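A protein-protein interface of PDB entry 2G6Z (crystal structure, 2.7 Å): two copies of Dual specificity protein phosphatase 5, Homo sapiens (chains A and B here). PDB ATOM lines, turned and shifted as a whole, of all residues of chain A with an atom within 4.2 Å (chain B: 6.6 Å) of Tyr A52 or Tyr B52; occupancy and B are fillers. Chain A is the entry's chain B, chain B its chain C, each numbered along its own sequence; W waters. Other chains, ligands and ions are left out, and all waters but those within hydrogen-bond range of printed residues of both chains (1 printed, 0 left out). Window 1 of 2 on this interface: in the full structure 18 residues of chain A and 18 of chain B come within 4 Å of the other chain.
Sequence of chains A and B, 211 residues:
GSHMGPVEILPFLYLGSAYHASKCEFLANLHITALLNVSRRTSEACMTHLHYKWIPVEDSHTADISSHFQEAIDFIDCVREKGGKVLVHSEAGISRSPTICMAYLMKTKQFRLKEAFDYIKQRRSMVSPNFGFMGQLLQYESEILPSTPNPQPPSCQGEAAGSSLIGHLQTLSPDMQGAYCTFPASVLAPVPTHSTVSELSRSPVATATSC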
ATOM      1  N   LEU A  35      -0.487  27.184   4.374  1.00  0.00           N
ATOM      2  CA  LEU A  35      -1.896  27.525   4.308  1.00  0.00           C
ATOM      3  C   LEU A  35      -2.613  26.422   3.567  1.00  0.00           C
ATOM      4  O   LEU A  35      -2.097  25.868   2.599  1.00  0.00           O
ATOM      5  CB  LEU A  35      -2.115  28.841   3.557  1.00  0.00           C
ATOM      6  CG  LEU A  35      -1.354  30.063   4.079  1.00  0.00           C
ATOM      7  CD1 LEU A  35      -1.698  31.291   3.239  1.00  0.00           C
ATOM      8  CD2 LEU A  35      -1.705  30.294   5.536  1.00  0.00           C
ATOM      9  N   ASN A  37      -6.231  26.145   1.943  1.00  0.00           N
ATOM     10  CA  ASN A  37      -7.450  26.856   1.589  1.00  0.00           C
ATOM     11  C   ASN A  37      -8.551  25.919   1.116  1.00  0.00           C
ATOM     12  O   ASN A  37      -8.424  25.288   0.068  1.00  0.00           O
ATOM     13  CB  ASN A  37      -7.150  27.897   0.505  1.00  0.00           C
ATOM     14  CG  ASN A  37      -8.385  28.694   0.101  1.00  0.00           C
ATOM     15  OD1 ASN A  37      -9.254  28.967   0.924  1.00  0.00           O
ATOM     16  ND2 ASN A  37      -8.457  29.079  -1.166  1.00  0.00           N
ATOM     17  N   THR A  42      -9.243  31.848  -4.589  1.00  0.00           N
ATOM     18  CA  THR A  42      -7.868  31.954  -4.128  1.00  0.00           C
ATOM     19  C   THR A  42      -7.559  33.422  -3.914  1.00  0.00           C
ATOM     20  O   THR A  42      -8.031  34.281  -4.660  1.00  0.00           O
ATOM     21  CB  THR A  42      -6.864  31.384  -5.161  1.00  0.00           C
ATOM     22  OG1 THR A  42      -7.094  29.978  -5.336  1.00  0.00           O
ATOM     23  CG2 THR A  42      -5.425  31.611  -4.688  1.00  0.00           C
ATOM     24  N   MET A  47       0.770  34.647  -0.133  1.00  0.00           N
ATOM     25  CA  MET A  47       1.005  33.296  -0.651  1.00  0.00           C
ATOM     26  C   MET A  47       2.484  32.968  -0.872  1.00  0.00           C
ATOM     27  O   MET A  47       2.854  31.799  -1.052  1.00  0.00           O
ATOM     28  CB  MET A  47       0.265  33.085  -1.970  1.00  0.00           C
ATOM     29  CG  MET A  47      -1.179  32.694  -1.804  1.00  0.00           C
ATOM     30  SD  MET A  47      -1.917  32.188  -3.372  1.00  0.00           S
ATOM     31  CE  MET A  47      -1.187  30.569  -3.594  1.00  0.00           C
ATOM     32  N   LEU A  50       5.326  30.253   1.236  1.00  0.00           N
ATOM     33  CA  LEU A  50       4.500  29.423   2.111  1.00  0.00           C
ATOM     34  C   LEU A  50       3.972  28.151   1.448  1.00  0.00           C
ATOM     35  O   LEU A  50       3.481  28.194   0.314  1.00  0.00           O
ATOM     36  CB  LEU A  50       3.294  30.220   2.630  1.00  0.00           C
ATOM     37  CG  LEU A  50       3.452  31.425   3.560  1.00  0.00           C
ATOM     38  CD1 LEU A  50       2.063  31.991   3.860  1.00  0.00           C
ATOM     39  CD2 LEU A  50       4.155  31.026   4.855  1.00  0.00           C
ATOM     40  N   HIS A  51       4.073  27.026   2.156  1.00  0.00           N
ATOM     41  CA  HIS A  51       3.532  25.769   1.652  1.00  0.00           C
ATOM     42  C   HIS A  51       2.024  26.036   1.547  1.00  0.00           C
ATOM     43  O   HIS A  51       1.369  26.368   2.533  1.00  0.00           O
ATOM     44  CB  HIS A  51       3.805  24.624   2.638  1.00  0.00           C
ATOM     45  CG  HIS A  51       5.256  24.276   2.783  1.00  0.00           C
ATOM     46  ND1 HIS A  51       5.947  23.547   1.839  1.00  0.00           N
ATOM     47  CD2 HIS A  51       6.153  24.575   3.754  1.00  0.00           C
ATOM     48  CE1 HIS A  51       7.206  23.412   2.221  1.00  0.00           C
ATOM     49  NE2 HIS A  51       7.357  24.028   3.381  1.00  0.00           N
ATOM     50  N   TYR A  52       1.481  25.900   0.346  1.00  0.00           N
ATOM     51  CA  TYR A  52       0.073  26.176   0.090  1.00  0.00           C
ATOM     52  C   TYR A  52      -0.562  24.989  -0.629  1.00  0.00           C
ATOM     53  O   TYR A  52       0.033  24.399  -1.521  1.00  0.00           O
ATOM     54  CB  TYR A  52      -0.032  27.426  -0.796  1.00  0.00           C
ATOM     55  CG  TYR A  52      -1.434  27.867  -1.161  1.00  0.00           C
ATOM     56  CD1 TYR A  52      -2.143  28.750  -0.347  1.00  0.00           C
ATOM     57  CD2 TYR A  52      -2.042  27.430  -2.337  1.00  0.00           C
ATOM     58  CE1 TYR A  52      -3.420  29.197  -0.700  1.00  0.00           C
ATOM     59  CE2 TYR A  52      -3.321  27.867  -2.696  1.00  0.00           C
ATOM     60  CZ  TYR A  52      -3.998  28.754  -1.872  1.00  0.00           C
ATOM     61  OH  TYR A  52      -5.236  29.226  -2.234  1.00  0.00           O
ATOM     62  N   LYS A  53      -1.774  24.641  -0.229  1.00  0.00           N
ATOM     63  CA  LYS A  53      -2.510  23.538  -0.830  1.00  0.00           C
ATOM     64  C   LYS A  53      -3.918  24.068  -0.884  1.00  0.00           C
ATOM     65  O   LYS A  53      -4.435  24.562   0.120  1.00  0.00           O
ATOM     66  CB  LYS A  53      -2.455  22.291   0.056  1.00  0.00           C
ATOM     67  CG  LYS A  53      -3.575  21.287  -0.201  1.00  0.00           C
ATOM     68  CD  LYS A  53      -3.233  20.287  -1.301  1.00  0.00           C
ATOM     69  CE  LYS A  53      -2.166  19.273  -0.860  1.00  0.00           C
ATOM     70  NZ  LYS A  53      -1.988  18.202  -1.883  1.00  0.00           N
ATOM     71  N   TRP A  54      -4.528  23.976  -2.058  1.00  0.00           N
ATOM     72  CA  TRP A  54      -5.877  24.468  -2.257  1.00  0.00           C
ATOM     73  C   TRP A  54      -6.823  23.332  -2.623  1.00  0.00           C
ATOM     74  O   TRP A  54      -6.672  22.709  -3.668  1.00  0.00           O
ATOM     75  CB  TRP A  54      -5.854  25.530  -3.362  1.00  0.00           C
ATOM     76  CG  TRP A  54      -7.181  26.139  -3.702  1.00  0.00           C
ATOM     77  CD1 TRP A  54      -8.184  26.464  -2.834  1.00  0.00           C
ATOM     78  CD2 TRP A  54      -7.627  26.544  -4.998  1.00  0.00           C
ATOM     79  NE1 TRP A  54      -9.228  27.046  -3.511  1.00  0.00           N
ATOM     80  CE2 TRP A  54      -8.913  27.107  -4.842  1.00  0.00           C
ATOM     81  CE3 TRP A  54      -7.065  26.486  -6.280  1.00  0.00           C
ATOM     82  CZ2 TRP A  54      -9.648  27.611  -5.919  1.00  0.00           C
ATOM     83  CZ3 TRP A  54      -7.799  26.991  -7.353  1.00  0.00           C
ATOM     84  CH2 TRP A  54      -9.078  27.544  -7.163  1.00  0.00           C
ATOM     85  N   THR B  33       2.688  16.318  -8.407  1.00  0.00           N
ATOM     86  CA  THR B  33       1.921  16.611  -7.209  1.00  0.00           C
ATOM     87  C   THR B  33       2.166  18.000  -6.626  1.00  0.00           C
ATOM     88  O   THR B  33       1.364  18.481  -5.826  1.00  0.00           O
ATOM     89  CB  THR B  33       2.184  15.545  -6.112  1.00  0.00           C
ATOM     90  OG1 THR B  33       3.589  15.423  -5.871  1.00  0.00           O
ATOM     91  CG2 THR B  33       1.648  14.197  -6.552  1.00  0.00           C
ATOM     92  N   ALA B  34       3.254  18.653  -7.034  1.00  0.00           N
ATOM     93  CA  ALA B  34       3.575  19.979  -6.509  1.00  0.00           C
ATOM     94  C   ALA B  34       4.168  20.938  -7.522  1.00  0.00           C
ATOM     95  O   ALA B  34       4.886  20.547  -8.437  1.00  0.00           O
ATOM     96  CB  ALA B  34       4.518  19.860  -5.321  1.00  0.00           C
ATOM     97  N   LEU B  35       3.867  22.211  -7.328  1.00  0.00           N
ATOM     98  CA  LEU B  35       4.364  23.260  -8.188  1.00  0.00           C
ATOM     99  C   LEU B  35       5.171  24.251  -7.365  1.00  0.00           C
ATOM    100  O   LEU B  35       4.703  24.746  -6.343  1.00  0.00           O
ATOM    101  CB  LEU B  35       3.198  23.986  -8.866  1.00  0.00           C
ATOM    102  CG  LEU B  35       2.431  23.150  -9.894  1.00  0.00           C
ATOM    103  CD1 LEU B  35       1.150  23.851 -10.307  1.00  0.00           C
ATOM    104  CD2 LEU B  35       3.327  22.897 -11.095  1.00  0.00           C
ATOM    105  N   LEU B  36       6.400  24.508  -7.800  1.00  0.00           N
ATOM    106  CA  LEU B  36       7.271  25.476  -7.150  1.00  0.00           C
ATOM    107  C   LEU B  36       7.447  26.566  -8.202  1.00  0.00           C
ATOM    108  O   LEU B  36       8.221  26.421  -9.142  1.00  0.00           O
ATOM    109  CB  LEU B  36       8.614  24.848  -6.793  1.00  0.00           C
ATOM    110  CG  LEU B  36       9.675  25.838  -6.303  1.00  0.00           C
ATOM    111  CD1 LEU B  36       9.130  26.626  -5.126  1.00  0.00           C
ATOM    112  CD2 LEU B  36      10.944  25.101  -5.910  1.00  0.00           C
ATOM    113  N   ASN B  37       6.696  27.646  -8.047  1.00  0.00           N
ATOM    114  CA  ASN B  37       6.726  28.758  -8.983  1.00  0.00           C
ATOM    115  C   ASN B  37       7.758  29.819  -8.590  1.00  0.00           C
ATOM    116  O   ASN B  37       7.703  30.375  -7.488  1.00  0.00           O
ATOM    117  CB  ASN B  37       5.333  29.374  -9.059  1.00  0.00           C
ATOM    118  CG  ASN B  37       5.276  30.565  -9.969  1.00  0.00           C
ATOM    119  OD1 ASN B  37       6.039  30.663 -10.938  1.00  0.00           O
ATOM    120  ND2 ASN B  37       4.350  31.479  -9.687  1.00  0.00           N
ATOM    121  N   ARG B  41       4.539  36.220 -11.280  1.00  0.00           N
ATOM    122  CA  ARG B  41       3.107  36.171 -11.546  1.00  0.00           C
ATOM    123  C   ARG B  41       2.529  34.792 -11.228  1.00  0.00           C
ATOM    124  O   ARG B  41       3.092  33.762 -11.608  1.00  0.00           O
ATOM    125  CB  ARG B  41       2.808  36.530 -13.005  1.00  0.00           C
ATOM    126  CG  ARG B  41       3.313  37.903 -13.421  1.00  0.00           C
ATOM    127  CD  ARG B  41       2.476  38.477 -14.550  1.00  0.00           C
ATOM    128  NE  ARG B  41       3.268  39.328 -15.433  1.00  0.00           N
ATOM    129  CZ  ARG B  41       4.244  38.880 -16.221  1.00  0.00           C
ATOM    130  NH1 ARG B  41       4.551  37.588 -16.235  1.00  0.00           N
ATOM    131  NH2 ARG B  41       4.913  39.722 -17.002  1.00  0.00           N
ATOM    132  N   THR B  42       1.401  34.788 -10.523  1.00  0.00           N
ATOM    133  CA  THR B  42       0.717  33.559 -10.140  1.00  0.00           C
ATOM    134  C   THR B  42      -0.364  33.219 -11.148  1.00  0.00           C
ATOM    135  O   THR B  42      -0.986  34.101 -11.735  1.00  0.00           O
ATOM    136  CB  THR B  42       0.055  33.695  -8.741  1.00  0.00           C
ATOM    137  OG1 THR B  42       1.073  33.850  -7.742  1.00  0.00           O
ATOM    138  CG2 THR B  42      -0.795  32.463  -8.414  1.00  0.00           C
ATOM    139  N   SER B  43      -0.581  31.928 -11.353  1.00  0.00           N
ATOM    140  CA  SER B  43      -1.608  31.478 -12.272  1.00  0.00           C
ATOM    141  C   SER B  43      -2.350  30.346 -11.595  1.00  0.00           C
ATOM    142  O   SER B  43      -1.814  29.251 -11.413  1.00  0.00           O
ATOM    143  CB  SER B  43      -1.002  30.993 -13.589  1.00  0.00           C
ATOM    144  OG  SER B  43      -2.018  30.571 -14.483  1.00  0.00           O
ATOM    145  N   CYS B  46      -4.251  24.951 -12.827  1.00  0.00           N
ATOM    146  CA  CYS B  46      -3.812  23.675 -12.263  1.00  0.00           C
ATOM    147  C   CYS B  46      -3.241  23.808 -10.856  1.00  0.00           C
ATOM    148  O   CYS B  46      -2.195  23.236 -10.567  1.00  0.00           O
ATOM    149  CB  CYS B  46      -2.728  23.021 -13.129  1.00  0.00           C
ATOM    150  SG  CYS B  46      -2.866  23.208 -14.936  1.00  0.00           S
ATOM    151  N   MET B  47      -3.898  24.551  -9.975  1.00  0.00           N
ATOM    152  CA  MET B  47      -3.371  24.686  -8.623  1.00  0.00           C
ATOM    153  C   MET B  47      -4.073  23.796  -7.596  1.00  0.00           C
ATOM    154  O   MET B  47      -3.536  23.556  -6.510  1.00  0.00           O
ATOM    155  CB  MET B  47      -3.447  26.142  -8.158  1.00  0.00           C
ATOM    156  CG  MET B  47      -2.221  26.972  -8.466  1.00  0.00           C
ATOM    157  SD  MET B  47      -2.297  28.578  -7.637  1.00  0.00           S
ATOM    158  CE  MET B  47      -1.834  28.124  -5.952  1.00  0.00           C
ATOM    159  N   LEU B  50      -2.737  20.494  -5.060  1.00  0.00           N
ATOM    160  CA  LEU B  50      -1.305  20.420  -5.280  1.00  0.00           C
ATOM    161  C   LEU B  50      -0.479  21.257  -4.319  1.00  0.00           C
ATOM    162  O   LEU B  50      -0.800  22.414  -4.057  1.00  0.00           O
ATOM    163  CB  LEU B  50      -0.973  20.860  -6.712  1.00  0.00           C
ATOM    164  CG  LEU B  50      -1.547  20.089  -7.904  1.00  0.00           C
ATOM    165  CD1 LEU B  50      -0.999  20.697  -9.202  1.00  0.00           C
ATOM    166  CD2 LEU B  50      -1.165  18.600  -7.802  1.00  0.00           C
ATOM    167  N   HIS B  51       0.588  20.656  -3.804  1.00  0.00           N
ATOM    168  CA  HIS B  51       1.506  21.362  -2.925  1.00  0.00           C
ATOM    169  C   HIS B  51       2.106  22.483  -3.794  1.00  0.00           C
ATOM    170  O   HIS B  51       2.768  22.215  -4.794  1.00  0.00           O
ATOM    171  CB  HIS B  51       2.612  20.418  -2.439  1.00  0.00           C
ATOM    172  CG  HIS B  51       2.107  19.264  -1.631  1.00  0.00           C
ATOM    173  ND1 HIS B  51       1.559  19.416  -0.375  1.00  0.00           N
ATOM    174  CD2 HIS B  51       2.048  17.938  -1.906  1.00  0.00           C
ATOM    175  CE1 HIS B  51       1.186  18.235   0.088  1.00  0.00           C
ATOM    176  NE2 HIS B  51       1.470  17.321  -0.823  1.00  0.00           N
ATOM    177  N   TYR B  52       1.847  23.730  -3.406  1.00  0.00           N
ATOM    178  CA  TYR B  52       2.316  24.904  -4.124  1.00  0.00           C
ATOM    179  C   TYR B  52       3.179  25.780  -3.226  1.00  0.00           C
ATOM    180  O   TYR B  52       2.889  25.934  -2.042  1.00  0.00           O
ATOM    181  CB  TYR B  52       1.113  25.720  -4.580  1.00  0.00           C
ATOM    182  CG  TYR B  52       1.434  26.936  -5.427  1.00  0.00           C
ATOM    183  CD1 TYR B  52       1.654  26.811  -6.797  1.00  0.00           C
ATOM    184  CD2 TYR B  52       1.464  28.219  -4.870  1.00  0.00           C
ATOM    185  CE1 TYR B  52       1.887  27.929  -7.601  1.00  0.00           C
ATOM    186  CE2 TYR B  52       1.699  29.349  -5.671  1.00  0.00           C
ATOM    187  CZ  TYR B  52       1.907  29.191  -7.038  1.00  0.00           C
ATOM    188  OH  TYR B  52       2.134  30.279  -7.853  1.00  0.00           O
ATOM    189  N   LYS B  53       4.241  26.344  -3.793  1.00  0.00           N
ATOM    190  CA  LYS B  53       5.135  27.259  -3.075  1.00  0.00           C
ATOM    191  C   LYS B  53       5.527  28.331  -4.081  1.00  0.00           C
ATOM    192  O   LYS B  53       5.989  28.028  -5.184  1.00  0.00           O
ATOM    193  CB  LYS B  53       6.385  26.545  -2.576  1.00  0.00           C
ATOM    194  CG  LYS B  53       7.521  27.486  -2.174  1.00  0.00           C
ATOM    195  CD  LYS B  53       7.437  27.949  -0.727  1.00  0.00           C
ATOM    196  CE  LYS B  53       7.705  26.809   0.252  1.00  0.00           C
ATOM    197  NZ  LYS B  53       7.907  27.296   1.647  1.00  0.00           N
ATOM    198  N   TRP B  54       5.329  29.585  -3.703  1.00  0.00           N
ATOM    199  CA  TRP B  54       5.649  30.692  -4.587  1.00  0.00           C
ATOM    200  C   TRP B  54       6.822  31.471  -4.036  1.00  0.00           C
ATOM    201  O   TRP B  54       6.764  31.982  -2.922  1.00  0.00           O
ATOM    202  CB  TRP B  54       4.433  31.604  -4.721  1.00  0.00           C
ATOM    203  CG  TRP B  54       4.564  32.710  -5.737  1.00  0.00           C
ATOM    204  CD1 TRP B  54       5.407  32.753  -6.817  1.00  0.00           C
ATOM    205  CD2 TRP B  54       3.745  33.883  -5.827  1.00  0.00           C
ATOM    206  NE1 TRP B  54       5.154  33.878  -7.574  1.00  0.00           N
ATOM    207  CE2 TRP B  54       4.139  34.585  -6.988  1.00  0.00           C
ATOM    208  CE3 TRP B  54       2.710  34.405  -5.040  1.00  0.00           C
ATOM    209  CZ2 TRP B  54       3.534  35.783  -7.380  1.00  0.00           C
ATOM    210  CZ3 TRP B  54       2.108  35.596  -5.431  1.00  0.00           C
ATOM    211  CH2 TRP B  54       2.522  36.270  -6.591  1.00  0.00           C
ATOM    212  N   PHE B  75      11.837  22.527  -0.103  1.00  0.00           N
ATOM    213  CA  PHE B  75      10.550  22.225  -0.687  1.00  0.00           C
ATOM    214  C   PHE B  75      10.676  21.001  -1.578  1.00  0.00           C
ATOM    215  O   PHE B  75       9.907  20.057  -1.451  1.00  0.00           O
ATOM    216  CB  PHE B  75      10.037  23.402  -1.517  1.00  0.00           C
ATOM    217  CG  PHE B  75       8.623  23.220  -2.008  1.00  0.00           C
ATOM    218  CD1 PHE B  75       7.553  23.275  -1.120  1.00  0.00           C
ATOM    219  CD2 PHE B  75       8.363  22.964  -3.353  1.00  0.00           C
ATOM    220  CE1 PHE B  75       6.239  23.079  -1.568  1.00  0.00           C
ATOM    221  CE2 PHE B  75       7.059  22.766  -3.811  1.00  0.00           C
ATOM    222  CZ  PHE B  75       5.994  22.824  -2.920  1.00  0.00           C
ATOM    223  N   HIS B  89       9.105  25.765 -11.993  1.00  0.00           N
ATOM    224  CA  HIS B  89       8.966  26.558 -13.221  1.00  0.00           C
ATOM    225  C   HIS B  89       9.089  28.086 -13.076  1.00  0.00           C
ATOM    226  O   HIS B  89       8.976  28.650 -11.980  1.00  0.00           O
ATOM    227  CB  HIS B  89       7.620  26.255 -13.896  1.00  0.00           C
ATOM    228  CG  HIS B  89       6.437  26.752 -13.119  1.00  0.00           C
ATOM    229  ND1 HIS B  89       5.983  26.127 -11.979  1.00  0.00           N
ATOM    230  CD2 HIS B  89       5.682  27.867 -13.264  1.00  0.00           C
ATOM    231  CE1 HIS B  89       5.002  26.839 -11.450  1.00  0.00           C
ATOM    232  NE2 HIS B  89       4.802  27.900 -12.210  1.00  0.00           N
HETATM  233  O   HOH W   1       3.431  21.823   0.498  1.00  0.00           O
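Water W1 bridges a ring nitrogen (ND1) of His B51 and a ring nitrogen (ND1) of His A51.
Printed residues of chain B that touch a printed residue of chain A: Met B47, Leu B50, His B51, Tyr B52, Lys B53, Trp B54 and Phe B75. Among the printed residues, 14 pairs touch across the chains. Among the printed residues, no Asp or Glu carboxylate lies within 4 Å of a Lys or Arg side-chain nitrogen of the other chain.
Tyr A52 touches just these residues of chain B: Met B47 (3.6 Å), Leu B50 (3.3 Å), His B51 (3.6 Å) and Tyr B52 (2.7 Å). Of chain A, only Met A47 (3.8 Å), Leu A50 (3.3 Å), His A51 (3.7 Å) and Tyr A52 (2.7 Å) come within 4 Å of Tyr B52. Printed residues of chain A within 4 Å of Trp B54: Met A47 (3.999 Å). Of the printed residues of chain B, Met A47 touches Met B47 (3.5 Å), Tyr B52 (3.8 Å) and Trp B54 (3.999 Å). Printed residues of chain B within 4 Å of His A51: Tyr B52 (3.7 Å), Lys B53 (3.7 Å) and Phe B75 (3.4 Å). The nearest printed residue of chain A that does not touch Tyr B52 is Lys A53 (4.9 Å). The nearest printed residue of chain A that does not touch Phe B75 is Tyr A52 (5.9 Å).
Among the printed residues, merely in contact across the chains: Met A47 with Met B47, Met A47 with Tyr B52, Met A47 with Trp B54, Leu A50 with Lys B53, His A51 with Tyr B52, His A51 with Lys B53, His A51 with Phe B75, Tyr A52 with Met B47, Tyr A52 with His B51, Lys A53 with Leu B50 and Lys A53 with His B51.
The backbone carbonyl oxygen (O) of Tyr A52 is in hydrogen-bond range of the backbone NH (N) of Tyr B52. The backbone carbonyl oxygen (O) of Tyr B52 lies close to the backbone carbonyl oxygen (O) of Leu A50, at 3.3 Å. The backbone carbonyl oxygen (O) of Leu B50 lies close to the backbone carbonyl oxygen (O) of Tyr A52.
Met B47 touches its own counterpart, Met A47. Met A47 touches Trp B54, but with the chains exchanged Trp A54 does not touch Met B47 (4.1 Å). Leu A50 touches Tyr B52, and with the chains exchanged Tyr A52 touches Leu B50. Tyr A52 touches its own counterpart, Tyr B52. Of the 14 pairs that touch across the chains among the printed residues, 12 have their exchanged pair printed and touching as well.
The backbone NH of Leu A35 sits at hydrogen-bond distance from the backbone carbonyl oxygen of His A51 (2.7 Å). OH of Tyr A52 sits at hydrogen-bond distance from ND2 of Asn A37 (3.4 Å). The backbone NH of Asn A37 is in hydrogen-bond range of the backbone carbonyl oxygen of Lys A53 (3.0 Å). O of Thr B33 is in hydrogen-bond range of N of His B51, at 3.1 Å. The backbone NH (N) of Leu B35 lies within hydrogen-bond range of the backbone carbonyl oxygen (O) of His B51, 2.8 Å away. N of Asn B37 sits at hydrogen-bond distance from O of Lys B53.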
